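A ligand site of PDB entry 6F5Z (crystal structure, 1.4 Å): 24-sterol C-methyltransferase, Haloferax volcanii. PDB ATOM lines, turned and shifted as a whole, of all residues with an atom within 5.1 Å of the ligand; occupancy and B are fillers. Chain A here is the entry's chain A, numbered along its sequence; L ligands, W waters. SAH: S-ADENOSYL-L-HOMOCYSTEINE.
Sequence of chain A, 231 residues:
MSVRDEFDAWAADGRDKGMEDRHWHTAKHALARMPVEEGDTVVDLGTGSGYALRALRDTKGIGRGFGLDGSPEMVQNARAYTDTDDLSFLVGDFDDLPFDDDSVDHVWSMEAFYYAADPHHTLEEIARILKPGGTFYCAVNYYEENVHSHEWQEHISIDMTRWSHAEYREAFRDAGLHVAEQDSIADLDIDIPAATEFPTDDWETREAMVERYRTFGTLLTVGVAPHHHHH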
ATOM      1  N   PHE A   7       9.451   1.578  10.476  1.00  0.00           N
ATOM      2  CA  PHE A   7       8.198   1.956   9.781  1.00  0.00           C
ATOM      3  C   PHE A   7       7.040   0.994  10.075  1.00  0.00           C
ATOM      4  O   PHE A   7       5.886   1.427  10.190  1.00  0.00           O
ATOM      5  CB  PHE A   7       8.434   2.045   8.267  1.00  0.00           C
ATOM      6  CG  PHE A   7       9.572   2.971   7.924  1.00  0.00           C
ATOM      7  CD1 PHE A   7       9.533   4.312   8.316  1.00  0.00           C
ATOM      8  CD2 PHE A   7      10.659   2.524   7.206  1.00  0.00           C
ATOM      9  CE1 PHE A   7      10.571   5.180   7.959  1.00  0.00           C
ATOM     10  CE2 PHE A   7      11.725   3.385   6.885  1.00  0.00           C
ATOM     11  CZ  PHE A   7      11.665   4.705   7.272  1.00  0.00           C
ATOM     12  N   TRP A  10       5.720   1.947  13.383  1.00  0.00           N
ATOM     13  CA  TRP A  10       4.913   3.194  13.336  1.00  0.00           C
ATOM     14  C   TRP A  10       3.530   2.913  12.815  1.00  0.00           C
ATOM     15  O   TRP A  10       2.566   3.528  13.274  1.00  0.00           O
ATOM     16  CB  TRP A  10       5.567   4.233  12.414  1.00  0.00           C
ATOM     17  CG  TRP A  10       6.965   4.648  12.802  1.00  0.00           C
ATOM     18  CD1 TRP A  10       7.648   4.319  13.940  1.00  0.00           C
ATOM     19  CD2 TRP A  10       7.798   5.544  12.063  1.00  0.00           C
ATOM     20  NE1 TRP A  10       8.887   4.938  13.925  1.00  0.00           N
ATOM     21  CE2 TRP A  10       9.010   5.677  12.782  1.00  0.00           C
ATOM     22  CE3 TRP A  10       7.633   6.254  10.865  1.00  0.00           C
ATOM     23  CZ2 TRP A  10      10.056   6.488  12.323  1.00  0.00           C
ATOM     24  CZ3 TRP A  10       8.693   7.042  10.399  1.00  0.00           C
ATOM     25  CH2 TRP A  10       9.886   7.145  11.124  1.00  0.00           C
ATOM     26  N   ASP A  16       1.622   6.602  11.868  1.00  0.00           N
ATOM     27  CA  ASP A  16       1.272   6.913  10.473  1.00  0.00           C
ATOM     28  C   ASP A  16       0.301   8.135  10.473  1.00  0.00           C
ATOM     29  O   ASP A  16       0.484   9.054   9.662  1.00  0.00           O
ATOM     30  CB  ASP A  16       0.591   5.698   9.785  1.00  0.00           C
ATOM     31  CG  ASP A  16      -0.557   5.011  10.537  1.00  0.00           C
ATOM     32  OD1 ASP A  16      -0.696   5.227  11.748  1.00  0.00           O
ATOM     33  OD2 ASP A  16      -1.315   4.254   9.889  1.00  0.00           O
ATOM     34  N   MET A  19       2.168  11.311  11.718  1.00  0.00           N
ATOM     35  CA  MET A  19       2.966  11.893  10.628  1.00  0.00           C
ATOM     36  C   MET A  19       2.035  12.630   9.665  1.00  0.00           C
ATOM     37  O   MET A  19       2.411  13.707   9.165  1.00  0.00           O
ATOM     38  CB  MET A  19       3.647  10.775   9.875  1.00  0.00           C
ATOM     39  CG  MET A  19       4.906  10.265  10.535  1.00  0.00           C
ATOM     40  SD  MET A  19       5.878   9.247   9.340  1.00  0.00           S
ATOM     41  CE  MET A  19       4.814   7.884   9.127  1.00  0.00           C
ATOM     42  N   GLU A  20       0.869  12.064   9.344  1.00  0.00           N
ATOM     43  CA  GLU A  20      -0.065  12.760   8.441  1.00  0.00           C
ATOM     44  C   GLU A  20      -0.419  14.161   8.981  1.00  0.00           C
ATOM     45  O   GLU A  20      -0.347  15.176   8.270  1.00  0.00           O
ATOM     46  CB  GLU A  20      -1.323  11.934   8.238  1.00  0.00           C
ATOM     47  CG  GLU A  20      -2.443  12.744   7.634  1.00  0.00           C
ATOM     48  CD  GLU A  20      -3.709  11.956   7.390  1.00  0.00           C
ATOM     49  OE1 GLU A  20      -3.648  10.698   7.293  1.00  0.00           O
ATOM     50  OE2 GLU A  20      -4.766  12.611   7.233  1.00  0.00           O
ATOM     51  N   HIS A  23       2.770  16.436   8.787  1.00  0.00           N
ATOM     52  CA  HIS A  23       3.296  16.676   7.433  1.00  0.00           C
ATOM     53  C   HIS A  23       2.323  17.424   6.567  1.00  0.00           C
ATOM     54  O   HIS A  23       2.748  18.113   5.640  1.00  0.00           O
ATOM     55  CB  HIS A  23       3.751  15.354   6.780  1.00  0.00           C
ATOM     56  CG  HIS A  23       4.853  14.693   7.536  1.00  0.00           C
ATOM     57  ND1 HIS A  23       5.077  13.323   7.440  1.00  0.00           N
ATOM     58  CD2 HIS A  23       5.775  15.227   8.383  1.00  0.00           C
ATOM     59  CE1 HIS A  23       6.110  13.067   8.235  1.00  0.00           C
ATOM     60  NE2 HIS A  23       6.546  14.176   8.844  1.00  0.00           N
ATOM     61  N   ASP A  44       2.595   7.782  -5.418  1.00  0.00           N
ATOM     62  CA  ASP A  44       3.021   8.366  -4.154  1.00  0.00           C
ATOM     63  C   ASP A  44       4.052   7.397  -3.572  1.00  0.00           C
ATOM     64  O   ASP A  44       3.686   6.262  -3.206  1.00  0.00           O
ATOM     65  CB  ASP A  44       1.791   8.498  -3.251  1.00  0.00           C
ATOM     66  CG  ASP A  44       1.990   9.039  -1.854  1.00  0.00           C
ATOM     67  OD1 ASP A  44       3.158   9.256  -1.477  1.00  0.00           O
ATOM     68  OD2 ASP A  44       0.974   9.173  -1.128  1.00  0.00           O
ATOM     69  N   GLY A  46       6.315   6.069  -0.792  1.00  0.00           N
ATOM     70  CA  GLY A  46       6.409   6.118   0.667  1.00  0.00           C
ATOM     71  C   GLY A  46       5.150   6.777   1.216  1.00  0.00           C
ATOM     72  O   GLY A  46       5.186   7.724   2.018  1.00  0.00           O
ATOM     73  N   THR A  47       4.000   6.230   0.783  1.00  0.00           N
ATOM     74  CA  THR A  47       2.705   6.846   1.008  1.00  0.00           C
ATOM     75  C   THR A  47       2.308   7.031   2.476  1.00  0.00           C
ATOM     76  O   THR A  47       1.508   7.917   2.783  1.00  0.00           O
ATOM     77  CB  THR A  47       1.646   6.072   0.219  1.00  0.00           C
ATOM     78  OG1 THR A  47       0.458   6.820   0.078  1.00  0.00           O
ATOM     79  CG2 THR A  47       1.309   4.705   0.794  1.00  0.00           C
ATOM     80  N   GLY A  48       2.832   6.210   3.384  1.00  0.00           N
ATOM     81  CA  GLY A  48       2.443   6.320   4.800  1.00  0.00           C
ATOM     82  C   GLY A  48       0.954   6.065   4.919  1.00  0.00           C
ATOM     83  O   GLY A  48       0.441   5.050   4.393  1.00  0.00           O
ATOM     84  N   SER A  49       0.231   7.051   5.509  1.00  0.00           N
ATOM     85  CA  SER A  49      -1.223   6.895   5.694  1.00  0.00           C
ATOM     86  C   SER A  49      -2.016   7.016   4.395  1.00  0.00           C
ATOM     87  O   SER A  49      -3.231   6.793   4.402  1.00  0.00           O
ATOM     88  CB  SER A  49      -1.760   7.911   6.693  1.00  0.00           C
ATOM     89  OG  SER A  49      -1.906   9.155   6.024  1.00  0.00           O
ATOM     90  N   TYR A  51      -2.482   9.888   2.785  1.00  0.00           N
ATOM     91  CA  TYR A  51      -3.202  11.154   2.708  1.00  0.00           C
ATOM     92  C   TYR A  51      -2.928  11.968   1.450  1.00  0.00           C
ATOM     93  O   TYR A  51      -3.819  12.705   1.005  1.00  0.00           O
ATOM     94  CB  TYR A  51      -2.962  12.040   3.958  1.00  0.00           C
ATOM     95  CG  TYR A  51      -1.566  12.628   4.020  1.00  0.00           C
ATOM     96  CD1 TYR A  51      -0.517  11.922   4.608  1.00  0.00           C
ATOM     97  CD2 TYR A  51      -1.270  13.849   3.416  1.00  0.00           C
ATOM     98  CE1 TYR A  51       0.788  12.432   4.616  1.00  0.00           C
ATOM     99  CE2 TYR A  51       0.030  14.347   3.394  1.00  0.00           C
ATOM    100  CZ  TYR A  51       1.056  13.629   3.967  1.00  0.00           C
ATOM    101  OH  TYR A  51       2.338  14.138   3.919  1.00  0.00           O
ATOM    102  N   LEU A  68       2.704   3.582  -2.901  1.00  0.00           N
ATOM    103  CA  LEU A  68       3.711   2.559  -2.706  1.00  0.00           C
ATOM    104  C   LEU A  68       4.385   2.725  -1.351  1.00  0.00           C
ATOM    105  O   LEU A  68       4.760   3.836  -0.991  1.00  0.00           O
ATOM    106  CB  LEU A  68       4.750   2.644  -3.856  1.00  0.00           C
ATOM    107  CG  LEU A  68       5.939   1.649  -3.817  1.00  0.00           C
ATOM    108  CD1 LEU A  68       6.469   1.391  -5.234  1.00  0.00           C
ATOM    109  CD2 LEU A  68       7.121   2.234  -2.936  1.00  0.00           C
ATOM    110  N   ASP A  69       4.604   1.626  -0.640  1.00  0.00           N
ATOM    111  CA  ASP A  69       5.326   1.745   0.641  1.00  0.00           C
ATOM    112  C   ASP A  69       6.042   0.427   0.866  1.00  0.00           C
ATOM    113  O   ASP A  69       5.528  -0.615   0.460  1.00  0.00           O
ATOM    114  CB  ASP A  69       4.358   2.039   1.798  1.00  0.00           C
ATOM    115  CG  ASP A  69       5.048   2.719   2.943  1.00  0.00           C
ATOM    116  OD1 ASP A  69       5.708   1.997   3.740  1.00  0.00           O
ATOM    117  OD2 ASP A  69       5.017   3.971   2.998  1.00  0.00           O
ATOM    118  N   GLY A  70       7.192   0.459   1.523  1.00  0.00           N
ATOM    119  CA  GLY A  70       7.943  -0.783   1.810  1.00  0.00           C
ATOM    120  C   GLY A  70       7.385  -1.538   3.005  1.00  0.00           C
ATOM    121  O   GLY A  70       7.808  -2.692   3.274  1.00  0.00           O
ATOM    122  N   SER A  71       6.446  -0.931   3.754  1.00  0.00           N
ATOM    123  CA  SER A  71       5.859  -1.542   4.942  1.00  0.00           C
ATOM    124  C   SER A  71       4.457  -2.102   4.625  1.00  0.00           C
ATOM    125  O   SER A  71       3.536  -1.317   4.415  1.00  0.00           O
ATOM    126  CB  SER A  71       5.748  -0.511   6.056  1.00  0.00           C
ATOM    127  OG  SER A  71       4.917  -1.025   7.089  1.00  0.00           O
ATOM    128  N   MET A  74       1.835  -0.480   6.786  1.00  0.00           N
ATOM    129  CA  MET A  74       1.570   0.891   6.394  1.00  0.00           C
ATOM    130  C   MET A  74       0.554   0.917   5.238  1.00  0.00           C
ATOM    131  O   MET A  74      -0.408   1.666   5.296  1.00  0.00           O
ATOM    132  CB  MET A  74       2.903   1.548   5.938  1.00  0.00           C
ATOM    133  CG  MET A  74       2.914   3.027   5.962  1.00  0.00           C
ATOM    134  SD  MET A  74       2.760   3.757   7.623  1.00  0.00           S
ATOM    135  CE  MET A  74       4.441   3.819   8.203  1.00  0.00           C
ATOM    136  N   GLY A  92       6.199  -2.074  -2.067  1.00  0.00           N
ATOM    137  CA  GLY A  92       7.258  -1.966  -3.036  1.00  0.00           C
ATOM    138  C   GLY A  92       8.437  -1.239  -2.461  1.00  0.00           C
ATOM    139  O   GLY A  92       8.364  -0.711  -1.333  1.00  0.00           O
ATOM    140  N   ASP A  93       9.540  -1.261  -3.188  1.00  0.00           N
ATOM    141  CA  ASP A  93      10.801  -0.679  -2.715  1.00  0.00           C
ATOM    142  C   ASP A  93      11.320   0.409  -3.661  1.00  0.00           C
ATOM    143  O   ASP A  93      11.267   0.289  -4.882  1.00  0.00           O
ATOM    144  CB  ASP A  93      11.862  -1.786  -2.568  1.00  0.00           C
ATOM    145  CG  ASP A  93      13.156  -1.259  -1.949  1.00  0.00           C
ATOM    146  OD1 ASP A  93      13.138  -0.876  -0.743  1.00  0.00           O
ATOM    147  OD2 ASP A  93      14.156  -1.193  -2.672  1.00  0.00           O
ATOM    148  N   PHE A  94      11.909   1.452  -3.056  1.00  0.00           N
ATOM    149  CA  PHE A  94      12.404   2.595  -3.820  1.00  0.00           C
ATOM    150  C   PHE A  94      13.522   2.237  -4.774  1.00  0.00           C
ATOM    151  O   PHE A  94      13.780   3.023  -5.685  1.00  0.00           O
ATOM    152  CB  PHE A  94      12.928   3.710  -2.883  1.00  0.00           C
ATOM    153  CG  PHE A  94      11.865   4.404  -2.037  1.00  0.00           C
ATOM    154  CD1 PHE A  94      10.502   4.240  -2.317  1.00  0.00           C
ATOM    155  CD2 PHE A  94      12.230   5.255  -1.001  1.00  0.00           C
ATOM    156  CE1 PHE A  94       9.533   4.878  -1.523  1.00  0.00           C
ATOM    157  CE2 PHE A  94      11.259   5.902  -0.217  1.00  0.00           C
ATOM    158  CZ  PHE A  94       9.930   5.686  -0.474  1.00  0.00           C
ATOM    159  N   MET A 110       6.803  12.646   0.050  1.00  0.00           N
ATOM    160  CA  MET A 110       6.985  13.526   1.209  1.00  0.00           C
ATOM    161  C   MET A 110       7.633  12.759   2.327  1.00  0.00           C
ATOM    162  O   MET A 110       7.146  11.690   2.710  1.00  0.00           O
ATOM    163  CB  MET A 110       5.628  14.046   1.698  1.00  0.00           C
ATOM    164  CG  MET A 110       5.668  14.803   3.053  1.00  0.00           C
ATOM    165  SD  MET A 110       6.577  16.367   2.928  1.00  0.00           S
ATOM    166  CE  MET A 110       6.184  17.085   4.480  1.00  0.00           C
ATOM    167  N   GLU A 111       8.736  13.302   2.873  1.00  0.00           N
ATOM    168  CA  GLU A 111       9.394  12.752   4.064  1.00  0.00           C
ATOM    169  C   GLU A 111       9.777  11.282   3.912  1.00  0.00           C
ATOM    170  O   GLU A 111       9.772  10.511   4.883  1.00  0.00           O
ATOM    171  CB  GLU A 111       8.455  12.956   5.288  1.00  0.00           C
ATOM    172  CG  GLU A 111       8.471  14.400   5.784  1.00  0.00           C
ATOM    173  CD  GLU A 111       9.750  14.648   6.547  1.00  0.00           C
ATOM    174  OE1 GLU A 111      10.828  14.757   5.918  1.00  0.00           O
ATOM    175  OE2 GLU A 111       9.694  14.601   7.801  1.00  0.00           O
ATOM    176  N   ALA A 112      10.214  10.946   2.695  1.00  0.00           N
ATOM    177  CA  ALA A 112      10.556   9.551   2.435  1.00  0.00           C
ATOM    178  C   ALA A 112      11.801   9.386   1.567  1.00  0.00           C
ATOM    179  O   ALA A 112      12.517   8.385   1.696  1.00  0.00           O
ATOM    180  CB  ALA A 112       9.390   8.845   1.761  1.00  0.00           C
ATOM    181  N   TYR A 115      15.323   8.156   2.696  1.00  0.00           N
ATOM    182  CA  TYR A 115      15.558   6.805   3.220  1.00  0.00           C
ATOM    183  C   TYR A 115      16.017   5.867   2.113  1.00  0.00           C
ATOM    184  O   TYR A 115      16.444   4.750   2.417  1.00  0.00           O
ATOM    185  CB  TYR A 115      14.295   6.209   3.855  1.00  0.00           C
ATOM    186  CG  TYR A 115      13.799   6.979   5.046  1.00  0.00           C
ATOM    187  CD1 TYR A 115      14.517   7.007   6.235  1.00  0.00           C
ATOM    188  CD2 TYR A 115      12.568   7.627   5.006  1.00  0.00           C
ATOM    189  CE1 TYR A 115      14.043   7.680   7.352  1.00  0.00           C
ATOM    190  CE2 TYR A 115      12.070   8.321   6.118  1.00  0.00           C
ATOM    191  CZ  TYR A 115      12.817   8.333   7.305  1.00  0.00           C
ATOM    192  OH  TYR A 115      12.376   9.005   8.405  1.00  0.00           O
ATOM    193  N   ALA A 116      15.931   6.281   0.829  1.00  0.00           N
ATOM    194  CA  ALA A 116      16.330   5.416  -0.276  1.00  0.00           C
ATOM    195  C   ALA A 116      17.761   4.952  -0.104  1.00  0.00           C
ATOM    196  O   ALA A 116      18.628   5.750   0.248  1.00  0.00           O
ATOM    197  CB  ALA A 116      16.165   6.139  -1.609  1.00  0.00           C
HETATM  198  N   SAH L   1       4.738  10.308   3.010  1.00  0.00           N
HETATM  199  CA  SAH L   1       4.170   9.978   4.348  1.00  0.00           C
HETATM  200  CB  SAH L   1       5.112   8.983   5.177  1.00  0.00           C
HETATM  201  CG  SAH L   1       6.528   9.523   5.394  1.00  0.00           C
HETATM  202  SD  SAH L   1       7.482   8.361   6.436  1.00  0.00           S
HETATM  203  C   SAH L   1       3.968  11.246   5.182  1.00  0.00           C
HETATM  204  O   SAH L   1       4.249  12.339   4.541  1.00  0.00           O
HETATM  205  OXT SAH L   1       3.607  11.198   6.320  1.00  0.00           O
HETATM  206  C5' SAH L   1       8.472   7.462   5.212  1.00  0.00           C
HETATM  207  C4' SAH L   1       7.672   6.367   4.523  1.00  0.00           C
HETATM  208  O4' SAH L   1       8.510   5.825   3.474  1.00  0.00           O
HETATM  209  C3' SAH L   1       7.265   5.203   5.435  1.00  0.00           C
HETATM  210  O3' SAH L   1       5.908   4.839   5.271  1.00  0.00           O
HETATM  211  C2' SAH L   1       8.243   4.089   5.017  1.00  0.00           C
HETATM  212  O2' SAH L   1       7.735   2.767   5.159  1.00  0.00           O
HETATM  213  C1' SAH L   1       8.512   4.416   3.551  1.00  0.00           C
HETATM  214  N9  SAH L   1       9.802   3.932   3.060  1.00  0.00           N
HETATM  215  C8  SAH L   1      11.036   4.238   3.555  1.00  0.00           C
HETATM  216  N7  SAH L   1      12.027   3.705   2.884  1.00  0.00           N
HETATM  217  C5  SAH L   1      11.400   3.003   1.861  1.00  0.00           C
HETATM  218  C6  SAH L   1      11.887   2.217   0.793  1.00  0.00           C
HETATM  219  N6  SAH L   1      13.196   1.970   0.576  1.00  0.00           N
HETATM  220  N1  SAH L   1      10.979   1.683  -0.056  1.00  0.00           N
HETATM  221  C2  SAH L   1       9.685   1.907   0.156  1.00  0.00           C
HETATM  222  N3  SAH L   1       9.108   2.608   1.134  1.00  0.00           N
HETATM  223  C4  SAH L   1      10.019   3.148   1.960  1.00  0.00           C
HETATM  224  O   HOH W   1      13.983   2.258   4.426  1.00  0.00           O
HETATM  225  O   HOH W   2      11.172  -1.515   1.093  1.00  0.00           O
HETATM  226  O   HOH W   3      15.573   2.251   2.301  1.00  0.00           O
HETATM  227  O   HOH W   4       1.655   9.204   6.976  1.00  0.00           O
HETATM  228  O   HOH W   5       9.288   0.536   4.625  1.00  0.00           O
HETATM  229  O   HOH W   6      15.809   2.189  -1.496  1.00  0.00           O
HETATM  230  O   HOH W   7       5.177  10.218   0.073  1.00  0.00           O
HETATM  231  O   HOH W   8       2.737  11.958   1.606  1.00  0.00           O
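SD of Met 19 sits close to SD of the ligand (3.4 Å).
The backbone carbonyl oxygen (O) of Glu 111 lies close to a sulfur (SD) of the ligand, 3.5 Å away.
Merely in contact with the ligand: Phe 7 (3.3 Å), Thr 47 (3.7 Å), Gly 48 (3.8 Å), Ser 71 (3.9 Å), Met 74 (3.4 Å), Gly 92 (3.3 Å), Ala 112 (3.6 Å) and Tyr 115 (3.5 Å).
The nearest printed residue that does not touch the ligand is Leu 68 (4.03 Å).
Water W5 bridges O2' of the ligand and N of Ser 71.
Water W4 lies within hydrogen-bond range of an oxygen (OXT) of the ligand (2.9 Å), the backbone carbonyl oxygen (O) of Asp 16 (2.9 Å) and the backbone NH (N) of Ser 49 (3.0 Å).
Water W8 lies within hydrogen-bond range of a nitrogen (N) of the ligand and the side-chain hydroxyl of Tyr 51.
Water W3 bridges O of Tyr 115 (2.6 Å) and N6 of the ligand (3.0 Å).
Water W7 lies within hydrogen-bond range of OD1 of Asp 44 (2.7 Å), N of Met 110 (2.9 Å), N of the ligand (3.0 Å) and O of Gly 46 (3.2 Å).
Water W2 lies within hydrogen-bond range of OD1 of Asp 93 (2.8 Å) and N1 of the ligand (3.4 Å).
N of Gly 48 lies within hydrogen-bond range of OD2 of Asp 69 (3.2 Å).
The backbone NH of Thr 47 lies within hydrogen-bond range of the side-chain carboxylate of Asp 69.
The backbone NH (N) of Tyr 51 sits close to the side-chain hydroxyl (OG) of Ser 49 (3.4 Å).
A ring nitrogen (ND1) of His 23 sits close to the backbone carbonyl oxygen (O) of Met 19 (3.2 Å).
The backbone carbonyl oxygen (O) of Gly 92 sits close to the backbone NH (N) of Gly 70 (3.3 Å).
The backbone NH (N) of Gly 46 sits at hydrogen-bond distance from the backbone carbonyl oxygen (O) of Leu 68, at 2.7 Å.
The backbone carbonyl oxygen (O) of Asp 69 lies within hydrogen-bond range of the backbone NH (N) of Gly 92, at 3.0 Å.
The backbone NH (N) of Met 74 sits at hydrogen-bond distance from the side-chain hydroxyl (OG) of Ser 71, at 3.1 Å.
A ring nitrogen (ND1) of His 23 lies within hydrogen-bond range of an oxygen (OXT) of the ligand (2.8 Å).
N6 of the ligand sits at hydrogen-bond distance from OD1 of Asp 93 (3.1 Å).
A nitrogen (N) of the ligand lies within hydrogen-bond range of the backbone carbonyl oxygen (O) of Gly 46 (2.8 Å).
A nitrogen (N1) of the ligand is in hydrogen-bond range of the backbone NH (N) of Phe 94 (3.1 Å).
O of the ligand lies within hydrogen-bond range of OH of Tyr 51 (2.7 Å).
A nitrogen (N) of the ligand sits at hydrogen-bond distance from the backbone carbonyl oxygen (O) of Met 110.
O3' of the ligand lies within hydrogen-bond range of OD2 of Asp 69 (2.6 Å).
N of Gly 70 sits at hydrogen-bond distance from N3 of the ligand (2.9 Å).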
